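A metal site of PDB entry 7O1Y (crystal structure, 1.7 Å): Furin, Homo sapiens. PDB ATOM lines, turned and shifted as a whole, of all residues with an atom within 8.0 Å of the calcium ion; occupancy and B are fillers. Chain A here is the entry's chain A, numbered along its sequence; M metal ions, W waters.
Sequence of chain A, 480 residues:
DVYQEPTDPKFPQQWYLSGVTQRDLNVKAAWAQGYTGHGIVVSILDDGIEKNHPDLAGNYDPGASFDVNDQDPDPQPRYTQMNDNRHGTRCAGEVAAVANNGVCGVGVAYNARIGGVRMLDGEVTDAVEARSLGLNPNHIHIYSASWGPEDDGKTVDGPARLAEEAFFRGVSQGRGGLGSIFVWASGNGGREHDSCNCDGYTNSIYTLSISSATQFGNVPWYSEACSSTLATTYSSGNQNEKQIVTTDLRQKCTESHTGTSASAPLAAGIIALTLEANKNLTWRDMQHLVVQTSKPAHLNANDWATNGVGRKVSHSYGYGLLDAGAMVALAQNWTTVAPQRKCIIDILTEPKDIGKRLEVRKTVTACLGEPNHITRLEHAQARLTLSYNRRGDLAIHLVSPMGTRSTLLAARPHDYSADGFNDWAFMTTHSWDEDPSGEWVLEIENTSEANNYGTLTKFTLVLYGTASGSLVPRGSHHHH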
ATOM      1  N   LYS A  51     -26.962   5.954  -7.709  1.00  0.00           N
ATOM      2  CA  LYS A  51     -28.174   5.429  -7.090  1.00  0.00           C
ATOM      3  C   LYS A  51     -27.877   4.673  -5.804  1.00  0.00           C
ATOM      4  O   LYS A  51     -28.793   4.490  -4.996  1.00  0.00           O
ATOM      5  CB  LYS A  51     -28.919   4.531  -8.092  1.00  0.00           C
ATOM      6  CG  LYS A  51     -28.201   3.260  -8.496  1.00  0.00           C
ATOM      7  CD  LYS A  51     -28.926   2.552  -9.650  1.00  0.00           C
ATOM      8  CE  LYS A  51     -28.198   1.283 -10.084  1.00  0.00           C
ATOM      9  NZ  LYS A  51     -26.853   1.556 -10.673  1.00  0.00           N
ATOM     10  N   PHE A  66     -33.296   6.779 -16.174  1.00  0.00           N
ATOM     11  CA  PHE A  66     -32.948   6.111 -17.411  1.00  0.00           C
ATOM     12  C   PHE A  66     -31.586   6.620 -17.838  1.00  0.00           C
ATOM     13  O   PHE A  66     -31.148   7.697 -17.425  1.00  0.00           O
ATOM     14  CB  PHE A  66     -33.982   6.371 -18.518  1.00  0.00           C
ATOM     15  CG  PHE A  66     -33.971   5.326 -19.588  1.00  0.00           C
ATOM     16  CD1 PHE A  66     -34.511   4.080 -19.359  1.00  0.00           C
ATOM     17  CD2 PHE A  66     -33.387   5.576 -20.820  1.00  0.00           C
ATOM     18  CE1 PHE A  66     -34.470   3.103 -20.342  1.00  0.00           C
ATOM     19  CE2 PHE A  66     -33.349   4.587 -21.791  1.00  0.00           C
ATOM     20  CZ  PHE A  66     -33.900   3.365 -21.547  1.00  0.00           C
ATOM     21  N   ASP A  67     -30.918   5.855 -18.694  1.00  0.00           N
ATOM     22  CA  ASP A  67     -29.655   6.274 -19.281  1.00  0.00           C
ATOM     23  C   ASP A  67     -29.870   6.459 -20.773  1.00  0.00           C
ATOM     24  O   ASP A  67     -29.858   5.495 -21.544  1.00  0.00           O
ATOM     25  CB  ASP A  67     -28.576   5.252 -18.977  1.00  0.00           C
ATOM     26  CG  ASP A  67     -27.194   5.660 -19.491  1.00  0.00           C
ATOM     27  OD1 ASP A  67     -27.108   6.567 -20.338  1.00  0.00           O
ATOM     28  OD2 ASP A  67     -26.198   5.045 -19.051  1.00  0.00           O
ATOM     29  N   VAL A  68     -30.092   7.705 -21.170  1.00  0.00           N
ATOM     30  CA  VAL A  68     -30.339   8.020 -22.575  1.00  0.00           C
ATOM     31  C   VAL A  68     -29.029   8.024 -23.346  1.00  0.00           C
ATOM     32  O   VAL A  68     -28.996   7.670 -24.527  1.00  0.00           O
ATOM     33  CB  VAL A  68     -31.065   9.369 -22.686  1.00  0.00           C
ATOM     34  CG1 VAL A  68     -31.241   9.775 -24.148  1.00  0.00           C
ATOM     35  CG2 VAL A  68     -32.416   9.263 -22.031  1.00  0.00           C
ATOM     36  N   ASN A  69     -27.909   8.391 -22.704  1.00  0.00           N
ATOM     37  CA  ASN A  69     -26.647   8.452 -23.441  1.00  0.00           C
ATOM     38  C   ASN A  69     -26.221   7.071 -23.930  1.00  0.00           C
ATOM     39  O   ASN A  69     -25.772   6.928 -25.073  1.00  0.00           O
ATOM     40  CB  ASN A  69     -25.559   9.052 -22.574  1.00  0.00           C
ATOM     41  CG  ASN A  69     -25.797  10.510 -22.254  1.00  0.00           C
ATOM     42  OD1 ASN A  69     -25.700  10.935 -21.098  1.00  0.00           O
ATOM     43  ND2 ASN A  69     -26.090  11.298 -23.283  1.00  0.00           N
ATOM     44  N   ASP A  70     -26.361   6.044 -23.086  1.00  0.00           N
ATOM     45  CA  ASP A  70     -25.953   4.687 -23.442  1.00  0.00           C
ATOM     46  C   ASP A  70     -27.144   3.782 -23.753  1.00  0.00           C
ATOM     47  O   ASP A  70     -26.950   2.612 -24.082  1.00  0.00           O
ATOM     48  CB  ASP A  70     -25.119   4.043 -22.317  1.00  0.00           C
ATOM     49  CG  ASP A  70     -23.672   4.505 -22.325  1.00  0.00           C
ATOM     50  OD1 ASP A  70     -23.261   5.133 -23.309  1.00  0.00           O
ATOM     51  OD2 ASP A  70     -22.973   4.256 -21.319  1.00  0.00           O
ATOM     52  N   GLN A  71     -28.357   4.295 -23.637  1.00  0.00           N
ATOM     53  CA  GLN A  71     -29.585   3.565 -23.964  1.00  0.00           C
ATOM     54  C   GLN A  71     -29.691   2.290 -23.121  1.00  0.00           C
ATOM     55  O   GLN A  71     -29.656   1.157 -23.614  1.00  0.00           O
ATOM     56  CB  GLN A  71     -29.664   3.271 -25.463  1.00  0.00           C
ATOM     57  CG  GLN A  71     -29.734   4.530 -26.342  1.00  0.00           C
ATOM     58  CD  GLN A  71     -30.148   4.259 -27.784  1.00  0.00           C
ATOM     59  N   ASP A  72     -29.840   2.503 -21.824  1.00  0.00           N
ATOM     60  CA  ASP A  72     -30.114   1.434 -20.873  1.00  0.00           C
ATOM     61  C   ASP A  72     -30.817   2.042 -19.672  1.00  0.00           C
ATOM     62  O   ASP A  72     -30.899   3.273 -19.552  1.00  0.00           O
ATOM     63  CB  ASP A  72     -28.810   0.692 -20.463  1.00  0.00           C
ATOM     64  CG  ASP A  72     -27.847   1.540 -19.621  1.00  0.00           C
ATOM     65  OD1 ASP A  72     -28.197   1.919 -18.481  1.00  0.00           O
ATOM     66  OD2 ASP A  72     -26.714   1.801 -20.087  1.00  0.00           O
ATOM     67  N   PRO A  73     -31.351   1.208 -18.779  1.00  0.00           N
ATOM     68  CA  PRO A  73     -32.164   1.731 -17.684  1.00  0.00           C
ATOM     69  C   PRO A  73     -31.359   2.280 -16.520  1.00  0.00           C
ATOM     70  O   PRO A  73     -31.954   2.935 -15.664  1.00  0.00           O
ATOM     71  CB  PRO A  73     -32.974   0.496 -17.217  1.00  0.00           C
ATOM     72  CG  PRO A  73     -32.740  -0.556 -18.239  1.00  0.00           C
ATOM     73  CD  PRO A  73     -31.387  -0.266 -18.824  1.00  0.00           C
ATOM     74  N   ASP A  74     -30.047   2.057 -16.484  1.00  0.00           N
ATOM     75  CA  ASP A  74     -29.232   2.311 -15.310  1.00  0.00           C
ATOM     76  C   ASP A  74     -28.497   3.631 -15.446  1.00  0.00           C
ATOM     77  O   ASP A  74     -27.581   3.731 -16.282  1.00  0.00           O
ATOM     78  CB  ASP A  74     -28.245   1.154 -15.119  1.00  0.00           C
ATOM     79  CG  ASP A  74     -27.345   1.331 -13.915  1.00  0.00           C
ATOM     80  OD1 ASP A  74     -27.436   2.342 -13.205  1.00  0.00           O
ATOM     81  OD2 ASP A  74     -26.515   0.423 -13.688  1.00  0.00           O
ATOM     82  N   PRO A  75     -28.855   4.677 -14.668  1.00  0.00           N
ATOM     83  CA  PRO A  75     -28.276   6.020 -14.855  1.00  0.00           C
ATOM     84  C   PRO A  75     -26.988   6.275 -14.084  1.00  0.00           C
ATOM     85  O   PRO A  75     -26.624   7.431 -13.840  1.00  0.00           O
ATOM     86  CB  PRO A  75     -29.379   6.930 -14.318  1.00  0.00           C
ATOM     87  CG  PRO A  75     -29.837   6.141 -13.107  1.00  0.00           C
ATOM     88  CD  PRO A  75     -29.903   4.700 -13.617  1.00  0.00           C
ATOM     89  N   GLN A  76     -26.325   5.207 -13.652  1.00  0.00           N
ATOM     90  CA  GLN A  76     -25.127   5.373 -12.850  1.00  0.00           C
ATOM     91  C   GLN A  76     -24.125   6.268 -13.579  1.00  0.00           C
ATOM     92  O   GLN A  76     -23.921   6.091 -14.791  1.00  0.00           O
ATOM     93  CB  GLN A  76     -24.474   4.017 -12.557  1.00  0.00           C
ATOM     94  CG  GLN A  76     -23.406   4.066 -11.455  1.00  0.00           C
ATOM     95  CD  GLN A  76     -24.020   4.052 -10.071  1.00  0.00           C
ATOM     96  OE1 GLN A  76     -25.206   3.775  -9.897  1.00  0.00           O
ATOM     97  NE2 GLN A  76     -23.207   4.330  -9.060  1.00  0.00           N
ATOM     98  N   PRO A  77     -23.514   7.239 -12.910  1.00  0.00           N
ATOM     99  CA  PRO A  77     -22.567   8.126 -13.591  1.00  0.00           C
ATOM    100  C   PRO A  77     -21.318   7.392 -14.054  1.00  0.00           C
ATOM    101  O   PRO A  77     -20.924   6.360 -13.496  1.00  0.00           O
ATOM    102  CB  PRO A  77     -22.211   9.179 -12.522  1.00  0.00           C
ATOM    103  CG  PRO A  77     -23.274   9.063 -11.468  1.00  0.00           C
ATOM    104  CD  PRO A  77     -23.724   7.633 -11.501  1.00  0.00           C
ATOM    105  N   ARG A  78     -20.708   7.947 -15.100  1.00  0.00           N
ATOM    106  CA  ARG A  78     -19.383   7.522 -15.550  1.00  0.00           C
ATOM    107  C   ARG A  78     -18.308   8.155 -14.659  1.00  0.00           C
ATOM    108  O   ARG A  78     -18.177   9.382 -14.585  1.00  0.00           O
ATOM    109  CB  ARG A  78     -19.208   7.923 -17.022  1.00  0.00           C
ATOM    110  CG  ARG A  78     -17.850   7.599 -17.656  1.00  0.00           C
ATOM    111  CD  ARG A  78     -17.829   7.917 -19.154  1.00  0.00           C
ATOM    112  NE  ARG A  78     -18.040   9.349 -19.402  1.00  0.00           N
ATOM    113  CZ  ARG A  78     -17.079  10.271 -19.488  1.00  0.00           C
ATOM    114  NH1 ARG A  78     -17.402  11.553 -19.689  1.00  0.00           N
ATOM    115  NH2 ARG A  78     -15.800   9.925 -19.377  1.00  0.00           N
ATOM    116  N   ARG A 118     -29.523  10.038 -17.129  1.00  0.00           N
ATOM    117  CA  ARG A 118     -28.178  10.256 -17.615  1.00  0.00           C
ATOM    118  C   ARG A 118     -28.322  10.648 -19.076  1.00  0.00           C
ATOM    119  O   ARG A 118     -28.578   9.797 -19.936  1.00  0.00           O
ATOM    120  CB  ARG A 118     -27.307   9.007 -17.435  1.00  0.00           C
ATOM    121  CG  ARG A 118     -25.869   9.194 -17.865  1.00  0.00           C
ATOM    122  CD  ARG A 118     -24.948   8.010 -17.461  1.00  0.00           C
ATOM    123  NE  ARG A 118     -23.639   8.179 -18.065  1.00  0.00           N
ATOM    124  CZ  ARG A 118     -23.172   7.496 -19.106  1.00  0.00           C
ATOM    125  NH1 ARG A 118     -21.975   7.812 -19.594  1.00  0.00           N
ATOM    126  NH2 ARG A 118     -23.856   6.484 -19.638  1.00  0.00           N
HETATM  127 CA    CA M   1     -25.985   3.016 -17.974  1.00  0.00          CA
HETATM  128  O   HOH W   1     -24.504   3.796 -16.296  1.00  0.00           O
HETATM  129  O   HOH W   2     -25.240   0.827 -16.973  1.00  0.00           O
HETATM  130  O   HOH W   3     -23.893   2.798 -19.143  1.00  0.00           O
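The guanidinium group (NH2) of Arg 118 is in salt-bridge range of the side-chain carboxylate (OD1) of Asp 67, at 3.3 Å. N of Asp 70 sits at hydrogen-bond distance from OD1 of Asp 67, at 2.9 Å. The side-chain carboxylate of Asp 74 is in hydrogen-bond range of the backbone NH of Gln 76, 3.1 Å away. The side-chain carboxylate of Asp 74 is in salt-bridge range of the side-chain amino group of Lys 51 (2.7 Å). The side-chain carboxylate of Asp 67 lies within hydrogen-bond range of the backbone NH of Asn 69, 3.1 Å away.
The nearest printed residue that does not touch the calcium ion is Arg 118 (4.4 Å).
The calcium ion is bound by OD2 of Asp 67 (2.3 Å), water W1 (2.4 Å), water W3 (2.4 Å), O of Asp 74 (2.4 Å), water W2 (2.5 Å), OD1 of Asp 72 (2.5 Å) and OD2 of Asp 72 (2.5 Å). The calcium ion has seven donor atoms within binding distance.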
